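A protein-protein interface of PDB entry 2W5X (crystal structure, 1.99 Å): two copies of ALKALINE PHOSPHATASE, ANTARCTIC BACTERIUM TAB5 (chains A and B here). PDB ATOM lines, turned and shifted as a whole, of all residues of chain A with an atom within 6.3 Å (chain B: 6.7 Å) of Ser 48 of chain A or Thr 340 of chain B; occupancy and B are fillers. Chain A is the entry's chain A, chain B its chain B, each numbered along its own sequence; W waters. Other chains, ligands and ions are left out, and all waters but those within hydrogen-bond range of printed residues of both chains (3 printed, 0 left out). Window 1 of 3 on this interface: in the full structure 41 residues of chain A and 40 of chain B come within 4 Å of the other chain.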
ATOM      1  N   ALA A  45      19.903 -16.918 -12.220  1.00  0.00           N
ATOM      2  CA  ALA A  45      18.446 -16.910 -12.355  1.00  0.00           C
ATOM      3  C   ALA A  45      17.953 -17.306 -13.743  1.00  0.00           C
ATOM      4  O   ALA A  45      18.033 -16.529 -14.682  1.00  0.00           O
ATOM      5  CB  ALA A  45      17.879 -15.554 -11.970  1.00  0.00           C
ATOM      6  N   GLY A  46      17.429 -18.520 -13.860  1.00  0.00           N
ATOM      7  CA  GLY A  46      16.743 -18.928 -15.068  1.00  0.00           C
ATOM      8  C   GLY A  46      15.298 -18.459 -14.998  1.00  0.00           C
ATOM      9  O   GLY A  46      14.894 -17.796 -14.039  1.00  0.00           O
ATOM     10  N   LEU A  47      14.513 -18.811 -16.007  1.00  0.00           N
ATOM     11  CA  LEU A  47      13.109 -18.418 -16.047  1.00  0.00           C
ATOM     12  C   LEU A  47      12.307 -18.957 -14.851  1.00  0.00           C
ATOM     13  O   LEU A  47      11.382 -18.304 -14.369  1.00  0.00           O
ATOM     14  CB  LEU A  47      12.477 -18.870 -17.359  1.00  0.00           C
ATOM     15  CG  LEU A  47      11.019 -18.475 -17.600  1.00  0.00           C
ATOM     16  CD1 LEU A  47      10.801 -16.975 -17.369  1.00  0.00           C
ATOM     17  CD2 LEU A  47      10.651 -18.882 -19.024  1.00  0.00           C
ATOM     18  N   SER A  48      12.666 -20.136 -14.360  1.00  0.00           N
ATOM     19  CA  SER A  48      12.002 -20.672 -13.172  1.00  0.00           C
ATOM     20  C   SER A  48      12.253 -19.804 -11.939  1.00  0.00           C
ATOM     21  O   SER A  48      11.325 -19.520 -11.177  1.00  0.00           O
ATOM     22  CB  SER A  48      12.439 -22.113 -12.909  1.00  0.00           C
ATOM     23  OG  SER A  48      12.151 -22.917 -14.039  1.00  0.00           O
ATOM     24  N   GLN A  49      13.500 -19.370 -11.750  1.00  0.00           N
ATOM     25  CA  GLN A  49      13.829 -18.475 -10.644  1.00  0.00           C
ATOM     26  C   GLN A  49      13.056 -17.161 -10.778  1.00  0.00           C
ATOM     27  O   GLN A  49      12.484 -16.660  -9.808  1.00  0.00           O
ATOM     28  CB  GLN A  49      15.340 -18.202 -10.583  1.00  0.00           C
ATOM     29  CG  GLN A  49      16.183 -19.338  -9.995  1.00  0.00           C
ATOM     30  CD  GLN A  49      16.612 -20.355 -11.031  1.00  0.00           C
ATOM     31  OE1 GLN A  49      16.093 -20.381 -12.143  1.00  0.00           O
ATOM     32  NE2 GLN A  49      17.569 -21.201 -10.670  1.00  0.00           N
ATOM     33  N   ILE A  50      13.042 -16.604 -11.984  1.00  0.00           N
ATOM     34  CA  ILE A  50      12.272 -15.385 -12.255  1.00  0.00           C
ATOM     35  C   ILE A  50      10.806 -15.614 -11.879  1.00  0.00           C
ATOM     36  O   ILE A  50      10.167 -14.779 -11.229  1.00  0.00           O
ATOM     37  CB  ILE A  50      12.377 -14.977 -13.744  1.00  0.00           C
ATOM     38  CG1 ILE A  50      13.778 -14.416 -14.051  1.00  0.00           C
ATOM     39  CG2 ILE A  50      11.300 -13.949 -14.102  1.00  0.00           C
ATOM     40  CD1 ILE A  50      14.198 -14.552 -15.499  1.00  0.00           C
ATOM     41  N   SER A  51      10.291 -16.775 -12.262  1.00  0.00           N
ATOM     42  CA  SER A  51       8.896 -17.115 -12.030  1.00  0.00           C
ATOM     43  C   SER A  51       8.503 -17.117 -10.545  1.00  0.00           C
ATOM     44  O   SER A  51       7.348 -16.848 -10.206  1.00  0.00           O
ATOM     45  CB  SER A  51       8.593 -18.469 -12.669  1.00  0.00           C
ATOM     46  OG  SER A  51       8.629 -18.373 -14.079  1.00  0.00           O
ATOM     47  N   SER A  52       9.445 -17.425  -9.655  1.00  0.00           N
ATOM     48  CA  SER A  52       9.124 -17.413  -8.223  1.00  0.00           C
ATOM     49  C   SER A  52       8.575 -16.058  -7.770  1.00  0.00           C
ATOM     50  O   SER A  52       7.693 -16.001  -6.914  1.00  0.00           O
ATOM     51  CB  SER A  52      10.315 -17.841  -7.355  1.00  0.00           C
ATOM     52  OG  SER A  52      11.415 -16.969  -7.507  1.00  0.00           O
ATOM     53  N   THR A  53       9.083 -14.967  -8.345  1.00  0.00           N
ATOM     54  CA  THR A  53       8.560 -13.645  -8.009  1.00  0.00           C
ATOM     55  C   THR A  53       7.059 -13.491  -8.311  1.00  0.00           C
ATOM     56  O   THR A  53       6.396 -12.642  -7.721  1.00  0.00           O
ATOM     57  CB  THR A  53       9.353 -12.491  -8.680  1.00  0.00           C
ATOM     58  OG1 THR A  53       9.048 -12.438 -10.076  1.00  0.00           O
ATOM     59  CG2 THR A  53      10.865 -12.684  -8.489  1.00  0.00           C
ATOM     60  N   TYR A  55       4.869 -15.848  -7.669  1.00  0.00           N
ATOM     61  CA  TYR A  55       4.141 -16.648  -6.678  1.00  0.00           C
ATOM     62  C   TYR A  55       4.539 -16.366  -5.225  1.00  0.00           C
ATOM     63  O   TYR A  55       3.769 -16.651  -4.304  1.00  0.00           O
ATOM     64  CB  TYR A  55       4.303 -18.149  -6.970  1.00  0.00           C
ATOM     65  CG  TYR A  55       3.703 -18.562  -8.291  1.00  0.00           C
ATOM     66  CD1 TYR A  55       4.468 -18.560  -9.454  1.00  0.00           C
ATOM     67  CD2 TYR A  55       2.368 -18.936  -8.379  1.00  0.00           C
ATOM     68  CE1 TYR A  55       3.921 -18.923 -10.660  1.00  0.00           C
ATOM     69  CE2 TYR A  55       1.812 -19.306  -9.584  1.00  0.00           C
ATOM     70  CZ  TYR A  55       2.589 -19.298 -10.719  1.00  0.00           C
ATOM     71  OH  TYR A  55       2.036 -19.660 -11.921  1.00  0.00           O
ATOM     72  N   GLU A 303      21.638 -20.309 -15.377  1.00  0.00           N
ATOM     73  CA  GLU A 303      20.721 -20.838 -14.372  1.00  0.00           C
ATOM     74  C   GLU A 303      21.521 -21.686 -13.387  1.00  0.00           C
ATOM     75  O   GLU A 303      22.560 -22.239 -13.750  1.00  0.00           O
ATOM     76  CB  GLU A 303      19.693 -21.745 -15.060  1.00  0.00           C
ATOM     77  CG  GLU A 303      18.435 -22.089 -14.244  1.00  0.00           C
ATOM     78  CD  GLU A 303      18.578 -23.309 -13.333  1.00  0.00           C
ATOM     79  OE1 GLU A 303      19.453 -24.174 -13.579  1.00  0.00           O
ATOM     80  OE2 GLU A 303      17.786 -23.405 -12.367  1.00  0.00           O
ATOM     81  N   GLY A 306      18.689 -26.138 -11.125  1.00  0.00           N
ATOM     82  CA  GLY A 306      17.498 -26.733 -11.702  1.00  0.00           C
ATOM     83  C   GLY A 306      16.267 -26.389 -10.880  1.00  0.00           C
ATOM     84  O   GLY A 306      15.330 -27.176 -10.790  1.00  0.00           O
ATOM     85  N   PHE A 307      16.278 -25.210 -10.268  1.00  0.00           N
ATOM     86  CA  PHE A 307      15.131 -24.714  -9.504  1.00  0.00           C
ATOM     87  C   PHE A 307      13.839 -24.955 -10.293  1.00  0.00           C
ATOM     88  O   PHE A 307      13.753 -24.599 -11.473  1.00  0.00           O
ATOM     89  CB  PHE A 307      15.325 -23.218  -9.208  1.00  0.00           C
ATOM     90  CG  PHE A 307      14.215 -22.599  -8.398  1.00  0.00           C
ATOM     91  CD1 PHE A 307      14.148 -22.793  -7.026  1.00  0.00           C
ATOM     92  CD2 PHE A 307      13.251 -21.814  -9.008  1.00  0.00           C
ATOM     93  CE1 PHE A 307      13.133 -22.227  -6.276  1.00  0.00           C
ATOM     94  CE2 PHE A 307      12.227 -21.244  -8.268  1.00  0.00           C
ATOM     95  CZ  PHE A 307      12.171 -21.452  -6.895  1.00  0.00           C
ATOM     96  N   THR A 308      12.844 -25.566  -9.644  1.00  0.00           N
ATOM     97  CA  THR A 308      11.581 -25.940 -10.298  1.00  0.00           C
ATOM     98  C   THR A 308      10.377 -25.637  -9.411  1.00  0.00           C
ATOM     99  O   THR A 308      10.385 -25.975  -8.229  1.00  0.00           O
ATOM    100  CB  THR A 308      11.566 -27.444 -10.627  1.00  0.00           C
ATOM    101  OG1 THR A 308      12.595 -27.727 -11.573  1.00  0.00           O
ATOM    102  CG2 THR A 308      10.205 -27.874 -11.206  1.00  0.00           C
ATOM    103  N   LEU A 309       9.352 -24.993  -9.968  1.00  0.00           N
ATOM    104  CA  LEU A 309       8.161 -24.657  -9.190  1.00  0.00           C
ATOM    105  C   LEU A 309       7.211 -25.854  -9.187  1.00  0.00           C
ATOM    106  O   LEU A 309       6.072 -25.771  -9.654  1.00  0.00           O
ATOM    107  CB  LEU A 309       7.469 -23.393  -9.730  1.00  0.00           C
ATOM    108  CG  LEU A 309       8.277 -22.087  -9.636  1.00  0.00           C
ATOM    109  CD1 LEU A 309       7.551 -20.923 -10.319  1.00  0.00           C
ATOM    110  CD2 LEU A 309       8.583 -21.734  -8.189  1.00  0.00           C
ATOM    111  N   GLY B  46       8.855 -26.330 -20.964  1.00  0.00           N
ATOM    112  CA  GLY B  46       9.363 -25.065 -20.458  1.00  0.00           C
ATOM    113  C   GLY B  46      10.571 -24.594 -21.265  1.00  0.00           C
ATOM    114  O   GLY B  46      10.956 -25.229 -22.250  1.00  0.00           O
ATOM    115  N   LEU B  47      11.186 -23.490 -20.856  1.00  0.00           N
ATOM    116  CA  LEU B  47      12.355 -22.973 -21.579  1.00  0.00           C
ATOM    117  C   LEU B  47      13.555 -23.940 -21.548  1.00  0.00           C
ATOM    118  O   LEU B  47      14.334 -23.997 -22.500  1.00  0.00           O
ATOM    119  CB  LEU B  47      12.748 -21.591 -21.054  1.00  0.00           C
ATOM    120  CG  LEU B  47      13.908 -20.859 -21.741  1.00  0.00           C
ATOM    121  CD1 LEU B  47      13.730 -20.774 -23.263  1.00  0.00           C
ATOM    122  CD2 LEU B  47      14.033 -19.476 -21.139  1.00  0.00           C
ATOM    123  N   SER B  48      13.702 -24.710 -20.472  1.00  0.00           N
ATOM    124  CA  SER B  48      14.751 -25.740 -20.428  1.00  0.00           C
ATOM    125  C   SER B  48      14.556 -26.803 -21.520  1.00  0.00           C
ATOM    126  O   SER B  48      15.507 -27.148 -22.230  1.00  0.00           O
ATOM    127  CB  SER B  48      14.827 -26.393 -19.049  1.00  0.00           C
ATOM    128  OG  SER B  48      15.264 -25.477 -18.053  1.00  0.00           O
ATOM    129  N   ILE B  72       3.998 -16.397 -20.614  1.00  0.00           N
ATOM    130  CA  ILE B  72       2.678 -16.600 -20.015  1.00  0.00           C
ATOM    131  C   ILE B  72       2.737 -17.271 -18.644  1.00  0.00           C
ATOM    132  O   ILE B  72       3.574 -18.145 -18.390  1.00  0.00           O
ATOM    133  CB  ILE B  72       1.709 -17.404 -20.930  1.00  0.00           C
ATOM    134  CG1 ILE B  72       2.356 -18.715 -21.407  1.00  0.00           C
ATOM    135  CG2 ILE B  72       1.228 -16.542 -22.105  1.00  0.00           C
ATOM    136  CD1 ILE B  72       1.371 -19.710 -22.051  1.00  0.00           C
ATOM    137  N   LYS B  73       1.840 -16.838 -17.765  1.00  0.00           N
ATOM    138  CA  LYS B  73       1.675 -17.439 -16.459  1.00  0.00           C
ATOM    139  C   LYS B  73       0.528 -18.443 -16.598  1.00  0.00           C
ATOM    140  O   LYS B  73      -0.557 -18.100 -17.074  1.00  0.00           O
ATOM    141  CB  LYS B  73       1.341 -16.366 -15.418  1.00  0.00           C
ATOM    142  CG  LYS B  73       1.360 -16.874 -13.977  1.00  0.00           C
ATOM    143  CD  LYS B  73       0.870 -15.812 -13.002  1.00  0.00           C
ATOM    144  CE  LYS B  73       0.793 -16.376 -11.583  1.00  0.00           C
ATOM    145  NZ  LYS B  73       0.441 -15.343 -10.569  1.00  0.00           N
ATOM    146  N   THR B  74       0.774 -19.676 -16.176  1.00  0.00           N
ATOM    147  CA  THR B  74      -0.088 -20.797 -16.540  1.00  0.00           C
ATOM    148  C   THR B  74      -1.082 -21.296 -15.478  1.00  0.00           C
ATOM    149  O   THR B  74      -1.848 -22.214 -15.762  1.00  0.00           O
ATOM    150  CB  THR B  74       0.775 -21.992 -16.972  1.00  0.00           C
ATOM    151  OG1 THR B  74       1.622 -22.368 -15.879  1.00  0.00           O
ATOM    152  CG2 THR B  74       1.663 -21.611 -18.162  1.00  0.00           C
ATOM    153  N   HIS B 302       2.318 -25.643 -20.112  1.00  0.00           N
ATOM    154  CA  HIS B 302       3.030 -25.646 -18.831  1.00  0.00           C
ATOM    155  C   HIS B 302       4.340 -26.419 -19.013  1.00  0.00           C
ATOM    156  O   HIS B 302       4.608 -26.935 -20.099  1.00  0.00           O
ATOM    157  CB  HIS B 302       2.193 -26.353 -17.775  1.00  0.00           C
ATOM    158  CG  HIS B 302       1.842 -27.752 -18.157  1.00  0.00           C
ATOM    159  ND1 HIS B 302       2.709 -28.809 -17.977  1.00  0.00           N
ATOM    160  CD2 HIS B 302       0.741 -28.262 -18.759  1.00  0.00           C
ATOM    161  CE1 HIS B 302       2.149 -29.915 -18.440  1.00  0.00           C
ATOM    162  NE2 HIS B 302       0.952 -29.612 -18.908  1.00  0.00           N
ATOM    163  N   GLU B 303       5.142 -26.506 -17.952  1.00  0.00           N
ATOM    164  CA  GLU B 303       6.389 -27.273 -17.973  1.00  0.00           C
ATOM    165  C   GLU B 303       6.172 -28.579 -17.225  1.00  0.00           C
ATOM    166  O   GLU B 303       5.320 -28.650 -16.338  1.00  0.00           O
ATOM    167  CB  GLU B 303       7.516 -26.484 -17.277  1.00  0.00           C
ATOM    168  CG  GLU B 303       8.930 -27.067 -17.433  1.00  0.00           C
ATOM    169  CD  GLU B 303       9.305 -28.147 -16.396  1.00  0.00           C
ATOM    170  OE1 GLU B 303       8.644 -28.249 -15.330  1.00  0.00           O
ATOM    171  OE2 GLU B 303      10.279 -28.902 -16.659  1.00  0.00           O
ATOM    172  N   THR B 304       6.941 -29.617 -17.546  1.00  0.00           N
ATOM    173  CA  THR B 304       6.872 -30.809 -16.696  1.00  0.00           C
ATOM    174  C   THR B 304       8.197 -31.515 -16.420  1.00  0.00           C
ATOM    175  O   THR B 304       9.076 -31.586 -17.278  1.00  0.00           O
ATOM    176  CB  THR B 304       5.747 -31.807 -17.125  1.00  0.00           C
ATOM    177  OG1 THR B 304       6.292 -33.112 -17.333  1.00  0.00           O
ATOM    178  CG2 THR B 304       5.077 -31.363 -18.373  1.00  0.00           C
ATOM    179  N   SER B 338       5.089 -28.178 -13.444  1.00  0.00           N
ATOM    180  CA  SER B 338       5.558 -27.067 -12.622  1.00  0.00           C
ATOM    181  C   SER B 338       4.977 -25.742 -13.106  1.00  0.00           C
ATOM    182  O   SER B 338       4.523 -25.628 -14.245  1.00  0.00           O
ATOM    183  CB  SER B 338       7.091 -27.005 -12.567  1.00  0.00           C
ATOM    184  OG  SER B 338       7.633 -26.523 -13.778  1.00  0.00           O
ATOM    185  N   ALA B 339       4.997 -24.744 -12.233  1.00  0.00           N
ATOM    186  CA  ALA B 339       4.337 -23.473 -12.502  1.00  0.00           C
ATOM    187  C   ALA B 339       5.259 -22.372 -13.039  1.00  0.00           C
ATOM    188  O   ALA B 339       4.951 -21.190 -12.889  1.00  0.00           O
ATOM    189  CB  ALA B 339       3.637 -22.980 -11.247  1.00  0.00           C
ATOM    190  N   THR B 340       6.377 -22.730 -13.664  1.00  0.00           N
ATOM    191  CA  THR B 340       7.220 -21.686 -14.263  1.00  0.00           C
ATOM    192  C   THR B 340       6.442 -20.933 -15.337  1.00  0.00           C
ATOM    193  O   THR B 340       5.505 -21.474 -15.935  1.00  0.00           O
ATOM    194  CB  THR B 340       8.517 -22.249 -14.879  1.00  0.00           C
ATOM    195  OG1 THR B 340       9.211 -21.205 -15.586  1.00  0.00           O
ATOM    196  CG2 THR B 340       8.206 -23.388 -15.840  1.00  0.00           C
ATOM    197  N   LEU B 341       6.807 -19.676 -15.568  1.00  0.00           N
ATOM    198  CA  LEU B 341       6.286 -18.959 -16.728  1.00  0.00           C
ATOM    199  C   LEU B 341       6.754 -19.680 -17.993  1.00  0.00           C
ATOM    200  O   LEU B 341       7.792 -20.355 -17.998  1.00  0.00           O
ATOM    201  CB  LEU B 341       6.766 -17.507 -16.749  1.00  0.00           C
ATOM    202  CG  LEU B 341       6.353 -16.570 -15.612  1.00  0.00           C
ATOM    203  CD1 LEU B 341       7.072 -15.233 -15.754  1.00  0.00           C
ATOM    204  CD2 LEU B 341       4.872 -16.360 -15.621  1.00  0.00           C
ATOM    205  N   ILE B 342       5.991 -19.524 -19.065  1.00  0.00           N
ATOM    206  CA  ILE B 342       6.251 -20.240 -20.311  1.00  0.00           C
ATOM    207  C   ILE B 342       6.489 -19.267 -21.472  1.00  0.00           C
ATOM    208  O   ILE B 342       5.719 -18.319 -21.657  1.00  0.00           O
ATOM    209  CB  ILE B 342       5.055 -21.166 -20.664  1.00  0.00           C
ATOM    210  CG1 ILE B 342       4.921 -22.295 -19.632  1.00  0.00           C
ATOM    211  CG2 ILE B 342       5.220 -21.738 -22.072  1.00  0.00           C
ATOM    212  CD1 ILE B 342       6.029 -23.352 -19.758  1.00  0.00           C
ATOM    213  N   PRO B 343       7.552 -19.496 -22.258  1.00  0.00           N
ATOM    214  CA  PRO B 343       7.836 -18.665 -23.434  1.00  0.00           C
ATOM    215  C   PRO B 343       6.725 -18.726 -24.480  1.00  0.00           C
ATOM    216  O   PRO B 343       6.146 -19.787 -24.704  1.00  0.00           O
ATOM    217  CB  PRO B 343       9.106 -19.304 -24.019  1.00  0.00           C
ATOM    218  CG  PRO B 343       9.705 -20.069 -22.920  1.00  0.00           C
ATOM    219  CD  PRO B 343       8.549 -20.567 -22.096  1.00  0.00           C
HETATM  220  O   HOH W   1       3.078 -19.737 -14.601  1.00  0.00           O
HETATM  221  O   HOH W   2      11.789 -22.519 -16.803  1.00  0.00           O
HETATM  222  O   HOH W   3       9.542 -24.686 -12.833  1.00  0.00           O
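OG1 of Thr 340 of chain B is in hydrogen-bond range of OG of Ser 51 of chain A.
The side-chain hydroxyl of Ser 51 of chain A sits at hydrogen-bond distance from the backbone NH of Leu 341 of chain B, at 2.7 Å.
The side-chain hydroxyl (OH) of Tyr 55 of chain A sits close to the backbone carbonyl oxygen (O) of Ala 339 of chain B, at 3.4 Å.
N of Ala 339 of chain B sits at hydrogen-bond distance from O of Leu 309 of chain A.
The backbone carbonyl oxygen (O) of Leu 47 of chain A is in hydrogen-bond range of the side-chain hydroxyl (OG) of Ser 51 of chain A (2.8 Å).
The side-chain hydroxyl of Ser 48 of chain A sits close to the backbone carbonyl oxygen of Phe 307 of chain A, at 3.5 Å.
The side-chain hydroxyl (OG1) of Thr 308 of chain A is in hydrogen-bond range of the backbone carbonyl oxygen (O) of Gly 306 of chain A.
OE1 of Glu 303 of chain B lies within hydrogen-bond range of OG of Ser 338 of chain B (2.5 Å).
Leu 47 of chain A touches its own counterpart, Leu 47 of chain B.
Positions printed for both chains: 46, 47, 48 and 303.
Of the 15 printed residues of chain B, 6 touch a printed residue of chain A.
Printed residues of chain B that touch a printed residue of chain A: Leu 47, Lys 73, Ser 338, Ala 339, Thr 340 and Leu 341.
Hydrophobic or aromatic side chains of chain B within 4 Å of the printed part of chain A: Leu 47, Ala 339 and Leu 341.
Of the 15 printed residues of chain A, 6 touch a printed residue of chain B.
Among the printed residues, 12 pairs touch across the chains.
Among the printed residues, no Asp or Glu carboxylate lies within 4 Å of a Lys or Arg side-chain nitrogen of the other chain.
Of the printed residues of chain B, Leu 47 of chain A touches Leu 47 (3.98 Å), Thr 340 (3.8 Å) and Leu 341 (3.4 Å).
Of the printed residues of chain B, Tyr 55 of chain A touches Lys 73 (3.5 Å) and Ala 339 (3.3 Å).
Of the printed residues of chain B, Thr 308 of chain A touches Ser 338 (3.5 Å).
Ser 48 of chain B touches none of the printed residues of chain A.
Printed residues of chain A within 4 Å of Lys 73 of chain B: Tyr 55.
Of the printed residues of chain A, Ser 338 of chain B touches Thr 308 (3.5 Å) and Leu 309 (3.3 Å).
Thr 340 of chain B touches just these residues of chain A: Leu 47, Ser 48, Ser 51 and Leu 309.
Ile 342 of chain B touches none of the printed residues of chain A.
The nearest residue of chain A that does not touch Thr 340 of chain B is Tyr 55 of chain A (5.4 Å).
The nearest printed residue of chain A that does not touch Leu 47 of chain B is Gly 46 of chain A (6.4 Å).
Water W1 lies within hydrogen-bond range of the backbone NH of Thr 74 of chain B (2.8 Å), the side-chain hydroxyl of Tyr 55 of chain A (2.9 Å), the backbone carbonyl oxygen of Ala 339 of chain B (2.9 Å) and the backbone carbonyl oxygen of Thr 340 of chain B (3.3 Å).
Water W3 lies within hydrogen-bond range of the side-chain hydroxyl of Ser 338 of chain B, the backbone NH of Leu 309 of chain A and the side-chain hydroxyl of Ser 48 of chain A.
Water W2 bridges the side-chain hydroxyl (OG) of Ser 48 of chain A and the side-chain hydroxyl (OG1) of Thr 340 of chain B.
Leu 47 of chain A touches Leu 47 of chain B (CD2 to CB, 3.98 Å).
O of Leu 47 of chain A touches OG1 of Thr 340 of chain B (3.8 Å).
CD2 of Leu 47 of chain A touches O of Leu 341 of chain B (3.4 Å).
OG1 of Thr 340 of chain B touches CA of Ser 48 of chain A (3.7 Å).
Tyr 55 of chain A touches Lys 73 of chain B.
Thr 308 of chain A touches Ser 338 of chain B (CG2 to CB, 3.5 Å).
Leu 309 of chain A touches Ser 338 of chain B (O to CA, 3.3 Å).
CD1 of Leu 309 of chain A touches N of Thr 340 of chain B, 3.98 Å away.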
